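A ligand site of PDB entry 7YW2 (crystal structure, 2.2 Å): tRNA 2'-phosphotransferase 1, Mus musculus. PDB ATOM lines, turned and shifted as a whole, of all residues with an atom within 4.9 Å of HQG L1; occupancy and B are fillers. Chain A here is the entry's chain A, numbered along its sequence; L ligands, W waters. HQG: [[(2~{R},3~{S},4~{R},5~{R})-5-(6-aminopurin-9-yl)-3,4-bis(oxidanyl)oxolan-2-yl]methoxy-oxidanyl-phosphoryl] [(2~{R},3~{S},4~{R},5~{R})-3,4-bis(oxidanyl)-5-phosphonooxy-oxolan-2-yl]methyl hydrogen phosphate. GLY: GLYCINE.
ND1 of His 125 sits at hydrogen-bond distance from O of His 149.
The backbone carbonyl oxygen of Arg 145 sits at hydrogen-bond distance from the guanidinium group of Arg 142.
The guanidinium group of Arg 35 lies within hydrogen-bond range of the backbone carbonyl oxygen of Gln 99 (3.1 Å).
OG of Ser 141 sits at hydrogen-bond distance from OE1 of Gln 143 (3.3 Å).
OE1 of Gln 99 sits at hydrogen-bond distance from NE2 of His 149 (3.0 Å).
His 131 touches HQG L1.
CG1 of Ile 135 touches C5A of HQG L1, 3.3 Å away.
CA of Leu 140 touches N7A of HQG L1, 3.6 Å away.
Gln 143 touches HQG L1.
CB of His 149 touches O3D of HQG L1 (3.5 Å).
N of Ile 164 touches O3D of HQG L1 (3.5 Å).
18 residues have an atom within 4 Å of HQG L1: Arg 35, Lys 79, Arg 81, His 125, Thr 127, His 131, Ser 134, Ile 135, Gly 139, Leu 140, Ser 141, Gln 143, Arg 145, His 149, Ser 162, Gly 163, Ile 164 and Arg 165.
OG1 of Thr 127 lies within hydrogen-bond range of O2B of HQG L1, at 2.6 Å.
A ring nitrogen (NE2) of His 125 sits at hydrogen-bond distance from an oxygen (O2B) of HQG L1 (2.7 Å).
An oxygen (O2A) of HQG L1 is in salt-bridge range of the guanidinium group (NE) of Arg 145, 2.8 Å away.
The guanidinium group (NE) of Arg 165 is in salt-bridge range of an oxygen (O2N) of HQG L1 (2.8 Å).
The guanidinium group (NH2) of Arg 35 is in salt-bridge range of an oxygen (O2Z) of HQG L1 (2.8 Å).
An oxygen (O2Z) of HQG L1 is in salt-bridge range of the guanidinium group of Arg 81, 2.8 Å away.
A nitrogen (N1A) of HQG L1 sits at hydrogen-bond distance from the side-chain hydroxyl (OG) of Ser 134 (2.8 Å).
The backbone carbonyl oxygen (O) of Gly 139 lies within hydrogen-bond range of a nitrogen (N6A) of HQG L1, 2.9 Å away.
The backbone NH of Gly 163 lies within hydrogen-bond range of an oxygen (O2D) of HQG L1, at 3.0 Å.
The backbone carbonyl oxygen (O) of Gly 163 sits close to an oxygen (O3D) of HQG L1 (3.0 Å).
N of Ser 141 lies within hydrogen-bond range of N7A of HQG L1, 3.0 Å away.
The side-chain hydroxyl of Ser 162 lies within hydrogen-bond range of an oxygen (O2D) of HQG L1.
An oxygen (O1Z) of HQG L1 lies within salt-bridge range of the side-chain amino group of Lys 79 (3.0 Å).
ND1 of His 131 lies within hydrogen-bond range of OXT of GLY L2, 2.4 Å away.
Water W3 lies within hydrogen-bond range of an oxygen (O4D) of HQG L1 (2.6 Å), the side-chain amide oxygen of Gln 99 (2.9 Å) and the guanidinium group of Arg 35 (3.4 Å).
Water W9 lies within hydrogen-bond range of an oxygen (O3B) of HQG L1 (2.6 Å) and the backbone carbonyl oxygen (O) of Gly 126 (2.9 Å).
Water W1 lies within hydrogen-bond range of OG of Ser 162 (2.6 Å), NE2 of Gln 99 (2.7 Å) and O2Z of HQG L1 (2.9 Å).
Water W2 bridges an oxygen (O2A) of HQG L1 and the backbone carbonyl oxygen (O) of Arg 142.
Water W4 lies within hydrogen-bond range of O1A of HQG L1 (2.9 Å) and NH2 of Arg 165 (3.4 Å).
Water W7 bridges N of His 149 (2.7 Å) and O1N of HQG L1 (3.1 Å).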
ATOM      1  N   ARG A  35     -24.785  -3.142  36.274  1.00  0.00           N
ATOM      2  CA  ARG A  35     -25.055  -1.743  35.892  1.00  0.00           C
ATOM      3  C   ARG A  35     -26.536  -1.397  35.898  1.00  0.00           C
ATOM      4  O   ARG A  35     -26.904  -0.276  36.263  1.00  0.00           O
ATOM      5  CB  ARG A  35     -24.505  -1.440  34.489  1.00  0.00           C
ATOM      6  CG  ARG A  35     -23.019  -1.235  34.367  1.00  0.00           C
ATOM      7  CD  ARG A  35     -22.628  -1.014  32.894  1.00  0.00           C
ATOM      8  NE  ARG A  35     -21.174  -0.938  32.698  1.00  0.00           N
ATOM      9  CZ  ARG A  35     -20.571  -1.042  31.526  1.00  0.00           C
ATOM     10  NH1 ARG A  35     -21.254  -1.203  30.402  1.00  0.00           N
ATOM     11  NH2 ARG A  35     -19.239  -1.011  31.475  1.00  0.00           N
ATOM     12  N   LYS A  79     -11.431  -3.223  28.896  1.00  0.00           N
ATOM     13  CA  LYS A  79     -11.919  -1.969  29.442  1.00  0.00           C
ATOM     14  C   LYS A  79     -11.901  -1.928  30.965  1.00  0.00           C
ATOM     15  O   LYS A  79     -12.346  -0.944  31.551  1.00  0.00           O
ATOM     16  CB  LYS A  79     -13.334  -1.689  28.910  1.00  0.00           C
ATOM     17  CG  LYS A  79     -13.442  -1.622  27.366  1.00  0.00           C
ATOM     18  CD  LYS A  79     -14.667  -0.851  26.892  1.00  0.00           C
ATOM     19  CE  LYS A  79     -14.810  -0.918  25.359  1.00  0.00           C
ATOM     20  NZ  LYS A  79     -15.901  -0.054  24.747  1.00  0.00           N
ATOM     21  N   ARG A  81     -13.762  -3.305  33.164  1.00  0.00           N
ATOM     22  CA  ARG A  81     -15.112  -2.942  33.559  1.00  0.00           C
ATOM     23  C   ARG A  81     -15.448  -3.247  35.024  1.00  0.00           C
ATOM     24  O   ARG A  81     -16.407  -2.653  35.548  1.00  0.00           O
ATOM     25  CB  ARG A  81     -16.108  -3.674  32.671  1.00  0.00           C
ATOM     26  CG  ARG A  81     -16.147  -3.144  31.249  1.00  0.00           C
ATOM     27  CD  ARG A  81     -17.064  -4.004  30.434  1.00  0.00           C
ATOM     28  NE  ARG A  81     -17.194  -3.542  29.063  1.00  0.00           N
ATOM     29  CZ  ARG A  81     -16.524  -4.068  28.039  1.00  0.00           C
ATOM     30  NH1 ARG A  81     -15.608  -5.006  28.223  1.00  0.00           N
ATOM     31  NH2 ARG A  81     -16.783  -3.635  26.802  1.00  0.00           N
ATOM     32  N   GLN A  99     -18.304   1.666  36.421  1.00  0.00           N
ATOM     33  CA  GLN A  99     -19.068   2.826  35.974  1.00  0.00           C
ATOM     34  C   GLN A  99     -20.173   2.321  35.059  1.00  0.00           C
ATOM     35  O   GLN A  99     -20.269   1.124  34.782  1.00  0.00           O
ATOM     36  CB  GLN A  99     -18.221   3.874  35.228  1.00  0.00           C
ATOM     37  CG  GLN A  99     -17.106   3.355  34.308  1.00  0.00           C
ATOM     38  CD  GLN A  99     -17.583   2.511  33.137  1.00  0.00           C
ATOM     39  OE1 GLN A  99     -18.526   2.865  32.391  1.00  0.00           O
ATOM     40  NE2 GLN A  99     -16.909   1.387  32.926  1.00  0.00           N
ATOM     41  N   HIS A 125     -15.857  13.509  24.303  1.00  0.00           N
ATOM     42  CA  HIS A 125     -16.979  12.590  24.238  1.00  0.00           C
ATOM     43  C   HIS A 125     -17.174  12.147  22.788  1.00  0.00           C
ATOM     44  O   HIS A 125     -17.358  13.001  21.902  1.00  0.00           O
ATOM     45  CB  HIS A 125     -18.276  13.221  24.756  1.00  0.00           C
ATOM     46  CG  HIS A 125     -19.475  12.326  24.608  1.00  0.00           C
ATOM     47  ND1 HIS A 125     -19.670  11.219  25.393  1.00  0.00           N
ATOM     48  CD2 HIS A 125     -20.508  12.359  23.734  1.00  0.00           C
ATOM     49  CE1 HIS A 125     -20.786  10.606  25.029  1.00  0.00           C
ATOM     50  NE2 HIS A 125     -21.318  11.286  24.029  1.00  0.00           N
ATOM     51  N   GLY A 126     -17.158  10.839  22.555  1.00  0.00           N
ATOM     52  CA  GLY A 126     -17.394  10.300  21.229  1.00  0.00           C
ATOM     53  C   GLY A 126     -18.865   9.935  21.063  1.00  0.00           C
ATOM     54  O   GLY A 126     -19.488   9.376  21.966  1.00  0.00           O
ATOM     55  N   THR A 127     -19.399  10.254  19.887  1.00  0.00           N
ATOM     56  CA  THR A 127     -20.804  10.041  19.631  1.00  0.00           C
ATOM     57  C   THR A 127     -21.015   9.912  18.120  1.00  0.00           C
ATOM     58  O   THR A 127     -20.055   9.681  17.376  1.00  0.00           O
ATOM     59  CB  THR A 127     -21.640  11.154  20.263  1.00  0.00           C
ATOM     60  OG1 THR A 127     -23.033  10.842  20.132  1.00  0.00           O
ATOM     61  CG2 THR A 127     -21.392  12.481  19.589  1.00  0.00           C
ATOM     62  N   PHE A 128     -22.256  10.061  17.671  1.00  0.00           N
ATOM     63  CA  PHE A 128     -22.664   9.653  16.335  1.00  0.00           C
ATOM     64  C   PHE A 128     -23.482  10.743  15.668  1.00  0.00           C
ATOM     65  O   PHE A 128     -24.088  11.588  16.331  1.00  0.00           O
ATOM     66  CB  PHE A 128     -23.456   8.347  16.402  1.00  0.00           C
ATOM     67  CG  PHE A 128     -22.724   7.233  17.100  1.00  0.00           C
ATOM     68  CD1 PHE A 128     -22.753   7.119  18.484  1.00  0.00           C
ATOM     69  CD2 PHE A 128     -21.988   6.318  16.375  1.00  0.00           C
ATOM     70  CE1 PHE A 128     -22.054   6.097  19.136  1.00  0.00           C
ATOM     71  CE2 PHE A 128     -21.285   5.301  17.014  1.00  0.00           C
ATOM     72  CZ  PHE A 128     -21.326   5.199  18.399  1.00  0.00           C
ATOM     73  N   HIS A 131     -27.154  11.633  16.748  1.00  0.00           N
ATOM     74  CA  HIS A 131     -27.408  12.448  17.934  1.00  0.00           C
ATOM     75  C   HIS A 131     -26.824  13.850  17.822  1.00  0.00           C
ATOM     76  O   HIS A 131     -27.001  14.662  18.745  1.00  0.00           O
ATOM     77  CB  HIS A 131     -26.806  11.793  19.181  1.00  0.00           C
ATOM     78  CG  HIS A 131     -27.230  10.375  19.410  1.00  0.00           C
ATOM     79  ND1 HIS A 131     -28.541   9.971  19.337  1.00  0.00           N
ATOM     80  CD2 HIS A 131     -26.516   9.292  19.775  1.00  0.00           C
ATOM     81  CE1 HIS A 131     -28.609   8.678  19.621  1.00  0.00           C
ATOM     82  NE2 HIS A 131     -27.384   8.243  19.887  1.00  0.00           N
ATOM     83  N   SER A 134     -29.117  17.034  18.130  1.00  0.00           N
ATOM     84  CA  SER A 134     -29.697  17.178  19.474  1.00  0.00           C
ATOM     85  C   SER A 134     -28.634  17.587  20.487  1.00  0.00           C
ATOM     86  O   SER A 134     -28.918  18.366  21.412  1.00  0.00           O
ATOM     87  CB  SER A 134     -30.365  15.866  19.900  1.00  0.00           C
ATOM     88  OG  SER A 134     -31.035  15.998  21.148  1.00  0.00           O
ATOM     89  N   ILE A 135     -27.422  17.067  20.356  1.00  0.00           N
ATOM     90  CA  ILE A 135     -26.339  17.444  21.249  1.00  0.00           C
ATOM     91  C   ILE A 135     -25.965  18.924  21.076  1.00  0.00           C
ATOM     92  O   ILE A 135     -25.824  19.660  22.061  1.00  0.00           O
ATOM     93  CB  ILE A 135     -25.140  16.496  21.040  1.00  0.00           C
ATOM     94  CG1 ILE A 135     -25.486  15.107  21.627  1.00  0.00           C
ATOM     95  CG2 ILE A 135     -23.881  17.061  21.673  1.00  0.00           C
ATOM     96  CD1 ILE A 135     -24.511  13.990  21.263  1.00  0.00           C
ATOM     97  N   LYS A 138     -29.068  20.866  22.767  1.00  0.00           N
ATOM     98  CA  LYS A 138     -29.328  20.803  24.200  1.00  0.00           C
ATOM     99  C   LYS A 138     -28.092  20.558  25.052  1.00  0.00           C
ATOM    100  O   LYS A 138     -28.174  20.634  26.285  1.00  0.00           O
ATOM    101  CB  LYS A 138     -30.366  19.707  24.498  1.00  0.00           C
ATOM    102  CG  LYS A 138     -31.546  19.686  23.522  1.00  0.00           C
ATOM    103  CD  LYS A 138     -32.845  19.275  24.236  1.00  0.00           C
ATOM    104  CE  LYS A 138     -33.839  18.580  23.283  1.00  0.00           C
ATOM    105  NZ  LYS A 138     -34.361  17.316  23.921  1.00  0.00           N
ATOM    106  N   GLY A 139     -26.951  20.249  24.440  1.00  0.00           N
ATOM    107  CA  GLY A 139     -25.801  19.758  25.190  1.00  0.00           C
ATOM    108  C   GLY A 139     -25.815  18.239  25.344  1.00  0.00           C
ATOM    109  O   GLY A 139     -26.763  17.549  24.961  1.00  0.00           O
ATOM    110  N   LEU A 140     -24.723  17.732  25.895  1.00  0.00           N
ATOM    111  CA  LEU A 140     -24.636  16.315  26.226  1.00  0.00           C
ATOM    112  C   LEU A 140     -25.550  16.000  27.383  1.00  0.00           C
ATOM    113  O   LEU A 140     -25.641  16.767  28.343  1.00  0.00           O
ATOM    114  CB  LEU A 140     -23.197  15.967  26.585  1.00  0.00           C
ATOM    115  CG  LEU A 140     -22.215  15.907  25.433  1.00  0.00           C
ATOM    116  CD1 LEU A 140     -20.894  15.441  25.998  1.00  0.00           C
ATOM    117  CD2 LEU A 140     -22.727  14.949  24.372  1.00  0.00           C
ATOM    118  N   SER A 141     -26.235  14.865  27.309  1.00  0.00           N
ATOM    119  CA  SER A 141     -27.139  14.418  28.366  1.00  0.00           C
ATOM    120  C   SER A 141     -26.674  13.068  28.898  1.00  0.00           C
ATOM    121  O   SER A 141     -26.231  12.213  28.130  1.00  0.00           O
ATOM    122  CB  SER A 141     -28.587  14.312  27.847  1.00  0.00           C
ATOM    123  OG  SER A 141     -29.482  13.965  28.884  1.00  0.00           O
ATOM    124  N   ARG A 142     -26.794  12.873  30.207  1.00  0.00           N
ATOM    125  CA  ARG A 142     -26.468  11.563  30.777  1.00  0.00           C
ATOM    126  C   ARG A 142     -27.372  10.457  30.253  1.00  0.00           C
ATOM    127  O   ARG A 142     -27.001   9.280  30.312  1.00  0.00           O
ATOM    128  CB  ARG A 142     -26.497  11.621  32.306  1.00  0.00           C
ATOM    129  CG  ARG A 142     -27.867  11.898  32.901  1.00  0.00           C
ATOM    130  CD  ARG A 142     -27.760  12.011  34.430  1.00  0.00           C
ATOM    131  NE  ARG A 142     -29.066  12.195  35.050  1.00  0.00           N
ATOM    132  CZ  ARG A 142     -29.976  11.227  35.165  1.00  0.00           C
ATOM    133  NH1 ARG A 142     -29.742   9.999  34.730  1.00  0.00           N
ATOM    134  NH2 ARG A 142     -31.157  11.515  35.721  1.00  0.00           N
ATOM    135  N   GLN A 143     -28.546  10.816  29.723  1.00  0.00           N
ATOM    136  CA  GLN A 143     -29.461   9.878  29.054  1.00  0.00           C
ATOM    137  C   GLN A 143     -29.901   8.849  30.097  1.00  0.00           C
ATOM    138  O   GLN A 143     -30.306   9.245  31.197  1.00  0.00           O
ATOM    139  CB  GLN A 143     -28.769   9.325  27.824  1.00  0.00           C
ATOM    140  CG  GLN A 143     -28.524  10.357  26.702  1.00  0.00           C
ATOM    141  CD  GLN A 143     -29.824  10.951  26.158  1.00  0.00           C
ATOM    142  OE1 GLN A 143     -30.576  11.613  26.876  1.00  0.00           O
ATOM    143  NE2 GLN A 143     -30.101  10.663  24.897  1.00  0.00           N
ATOM    144  N   ARG A 145     -28.279   6.924  31.987  1.00  0.00           N
ATOM    145  CA  ARG A 145     -27.263   6.550  32.955  1.00  0.00           C
ATOM    146  C   ARG A 145     -27.087   7.632  33.984  1.00  0.00           C
ATOM    147  O   ARG A 145     -27.647   8.726  33.901  1.00  0.00           O
ATOM    148  CB  ARG A 145     -25.926   6.245  32.288  1.00  0.00           C
ATOM    149  CG  ARG A 145     -25.992   5.330  31.110  1.00  0.00           C
ATOM    150  CD  ARG A 145     -24.608   4.912  30.698  1.00  0.00           C
ATOM    151  NE  ARG A 145     -24.607   4.209  29.414  1.00  0.00           N
ATOM    152  CZ  ARG A 145     -24.440   2.893  29.266  1.00  0.00           C
ATOM    153  NH1 ARG A 145     -24.190   2.115  30.315  1.00  0.00           N
ATOM    154  NH2 ARG A 145     -24.505   2.365  28.049  1.00  0.00           N
ATOM    155  N   HIS A 149     -20.413  10.042  29.965  1.00  0.00           N
ATOM    156  CA  HIS A 149     -19.136   9.339  29.879  1.00  0.00           C
ATOM    157  C   HIS A 149     -18.172  10.078  28.951  1.00  0.00           C
ATOM    158  O   HIS A 149     -18.500  10.301  27.771  1.00  0.00           O
ATOM    159  CB  HIS A 149     -19.335   7.891  29.410  1.00  0.00           C
ATOM    160  CG  HIS A 149     -19.806   6.985  30.501  1.00  0.00           C
ATOM    161  ND1 HIS A 149     -20.942   7.252  31.243  1.00  0.00           N
ATOM    162  CD2 HIS A 149     -19.282   5.844  30.997  1.00  0.00           C
ATOM    163  CE1 HIS A 149     -21.107   6.286  32.131  1.00  0.00           C
ATOM    164  NE2 HIS A 149     -20.107   5.428  32.015  1.00  0.00           N
ATOM    165  N   SER A 162     -11.012   2.804  28.389  1.00  0.00           N
ATOM    166  CA  SER A 162     -12.458   2.882  28.215  1.00  0.00           C
ATOM    167  C   SER A 162     -12.901   4.342  28.263  1.00  0.00           C
ATOM    168  O   SER A 162     -12.078   5.261  28.395  1.00  0.00           O
ATOM    169  CB  SER A 162     -13.175   2.041  29.281  1.00  0.00           C
ATOM    170  OG  SER A 162     -14.596   2.113  29.074  1.00  0.00           O
ATOM    171  N   GLY A 163     -14.217   4.550  28.112  1.00  0.00           N
ATOM    172  CA  GLY A 163     -14.795   5.875  28.150  1.00  0.00           C
ATOM    173  C   GLY A 163     -15.148   6.489  26.809  1.00  0.00           C
ATOM    174  O   GLY A 163     -15.748   7.574  26.772  1.00  0.00           O
ATOM    175  N   ILE A 164     -14.800   5.831  25.699  1.00  0.00           N
ATOM    176  CA  ILE A 164     -15.178   6.312  24.373  1.00  0.00           C
ATOM    177  C   ILE A 164     -15.350   5.099  23.469  1.00  0.00           C
ATOM    178  O   ILE A 164     -14.490   4.222  23.407  1.00  0.00           O
ATOM    179  CB  ILE A 164     -14.141   7.305  23.813  1.00  0.00           C
ATOM    180  CG1 ILE A 164     -14.553   7.787  22.435  1.00  0.00           C
ATOM    181  CG2 ILE A 164     -12.729   6.677  23.801  1.00  0.00           C
ATOM    182  CD1 ILE A 164     -13.824   9.029  22.010  1.00  0.00           C
ATOM    183  N   ARG A 165     -16.480   5.042  22.773  1.00  0.00           N
ATOM    184  CA  ARG A 165     -16.738   3.905  21.902  1.00  0.00           C
ATOM    185  C   ARG A 165     -15.790   3.936  20.703  1.00  0.00           C
ATOM    186  O   ARG A 165     -15.543   4.996  20.120  1.00  0.00           O
ATOM    187  CB  ARG A 165     -18.194   3.928  21.450  1.00  0.00           C
ATOM    188  CG  ARG A 165     -19.165   3.990  22.629  1.00  0.00           C
ATOM    189  CD  ARG A 165     -20.589   3.891  22.155  1.00  0.00           C
ATOM    190  NE  ARG A 165     -21.528   3.709  23.261  1.00  0.00           N
ATOM    191  CZ  ARG A 165     -21.771   2.546  23.859  1.00  0.00           C
ATOM    192  NH1 ARG A 165     -21.198   1.429  23.443  1.00  0.00           N
ATOM    193  NH2 ARG A 165     -22.608   2.511  24.894  1.00  0.00           N
ATOM    194  N   PHE A 203     -27.336  17.540  32.160  1.00  0.00           N
ATOM    195  CA  PHE A 203     -26.832  18.061  30.897  1.00  0.00           C
ATOM    196  C   PHE A 203     -25.482  18.746  31.070  1.00  0.00           C
ATOM    197  O   PHE A 203     -25.225  19.418  32.079  1.00  0.00           O
ATOM    198  CB  PHE A 203     -27.822  19.044  30.250  1.00  0.00           C
ATOM    199  CG  PHE A 203     -28.994  18.371  29.589  1.00  0.00           C
ATOM    200  CD1 PHE A 203     -30.110  18.020  30.322  1.00  0.00           C
ATOM    201  CD2 PHE A 203     -28.961  18.063  28.240  1.00  0.00           C
ATOM    202  CE1 PHE A 203     -31.180  17.397  29.720  1.00  0.00           C
ATOM    203  CE2 PHE A 203     -30.019  17.428  27.637  1.00  0.00           C
ATOM    204  CZ  PHE A 203     -31.137  17.098  28.371  1.00  0.00           C
HETATM  205  C1B HQG L   1     -25.878  10.538  23.119  1.00  0.00           C
HETATM  206  C1D HQG L   1     -19.037   2.160  26.929  1.00  0.00           C
HETATM  207  C2A HQG L   1     -29.370  12.921  21.916  1.00  0.00           C
HETATM  208  C2B HQG L   1     -24.667  10.179  23.558  1.00  0.00           C
HETATM  209  C2D HQG L   1     -18.064   3.381  26.602  1.00  0.00           C
HETATM  210  C3B HQG L   1     -24.728   8.651  23.407  1.00  0.00           C
HETATM  211  C3D HQG L   1     -18.709   4.416  26.844  1.00  0.00           C
HETATM  212  C4A HQG L   1     -27.424  12.415  23.110  1.00  0.00           C
HETATM  213  C4B HQG L   1     -26.246   8.292  23.720  1.00  0.00           C
HETATM  214  C4D HQG L   1     -19.840   3.977  27.973  1.00  0.00           C
HETATM  215  C5A HQG L   1     -27.522  13.582  23.756  1.00  0.00           C
HETATM  216  C5B HQG L   1     -26.337   7.551  25.062  1.00  0.00           C
HETATM  217  C5D HQG L   1     -20.984   4.984  27.903  1.00  0.00           C
HETATM  218  C6A HQG L   1     -28.557  14.446  23.481  1.00  0.00           C
HETATM  219  C8A HQG L   1     -25.749  12.571  24.488  1.00  0.00           C
HETATM  220  N1A HQG L   1     -29.464  14.115  22.574  1.00  0.00           N
HETATM  221  N3A HQG L   1     -28.347  12.078  22.187  1.00  0.00           N
HETATM  222  N6A HQG L   1     -28.877  15.753  24.030  1.00  0.00           N
HETATM  223  N7A HQG L   1     -26.492  13.671  24.607  1.00  0.00           N
HETATM  224  N9A HQG L   1     -26.315  11.799  23.565  1.00  0.00           N
HETATM  225  O1A HQG L   1     -24.560   4.275  26.023  1.00  0.00           O
HETATM  226  O1N HQG L   1     -21.186   7.547  26.266  1.00  0.00           O
HETATM  227  O1Z HQG L   1     -18.192  -0.872  26.542  1.00  0.00           O
HETATM  228  O2A HQG L   1     -25.769   5.907  27.544  1.00  0.00           O
HETATM  229  O2B HQG L   1     -23.565  10.693  22.717  1.00  0.00           O
HETATM  230  O2D HQG L   1     -16.882   3.241  27.535  1.00  0.00           O
HETATM  231  O2N HQG L   1     -22.198   6.154  24.415  1.00  0.00           O
HETATM  232  O2Z HQG L   1     -17.996  -0.840  28.979  1.00  0.00           O
HETATM  233  O3  HQG L   1     -23.519   6.603  26.615  1.00  0.00           O
HETATM  234  O3B HQG L   1     -24.427   8.288  22.159  1.00  0.00           O
HETATM  235  O3D HQG L   1     -17.855   5.472  27.393  1.00  0.00           O
HETATM  236  O3Z HQG L   1     -20.180  -0.383  27.927  1.00  0.00           O
HETATM  237  O4B HQG L   1     -26.863   9.427  23.819  1.00  0.00           O
HETATM  238  O4D HQG L   1     -20.236   2.799  27.632  1.00  0.00           O
HETATM  239  O4Z HQG L   1     -18.387   1.410  27.740  1.00  0.00           O
HETATM  240  O5B HQG L   1     -25.604   6.351  24.963  1.00  0.00           O
HETATM  241  O5D HQG L   1     -21.407   4.970  26.565  1.00  0.00           O
HETATM  242  PA  HQG L   1     -24.889   5.716  26.325  1.00  0.00           P
HETATM  243  PN  HQG L   1     -22.048   6.353  25.899  1.00  0.00           P
HETATM  244  PZ  HQG L   1     -18.698  -0.215  27.796  1.00  0.00           P
HETATM  245  N   GLY L   2     -31.880   9.683  16.813  1.00  0.00           N
HETATM  246  CA  GLY L   2     -32.358  10.994  17.240  1.00  0.00           C
HETATM  247  C   GLY L   2     -31.579  11.401  18.495  1.00  0.00           C
HETATM  248  O   GLY L   2     -31.596  12.594  18.915  1.00  0.00           O
HETATM  249  OXT GLY L   2     -30.907  10.535  19.121  1.00  0.00           O
HETATM  250  O   HOH W   1     -16.001   0.547  30.530  1.00  0.00           O
HETATM  251  O   HOH W   2     -24.544   8.001  29.136  1.00  0.00           O
HETATM  252  O   HOH W   3     -20.114   1.968  30.135  1.00  0.00           O
HETATM  253  O   HOH W   4     -25.910   2.765  23.940  1.00  0.00           O
HETATM  254  O   HOH W   5     -23.823  11.218  26.820  1.00  0.00           O
HETATM  255  O   HOH W   6     -28.361   5.824  28.157  1.00  0.00           O
HETATM  256  O   HOH W   7     -22.547   9.243  28.455  1.00  0.00           O
HETATM  257  O   HOH W   8     -22.099  -0.183  26.291  1.00  0.00           O
HETATM  258  O   HOH W   9     -21.839   7.739  22.254  1.00  0.00           O
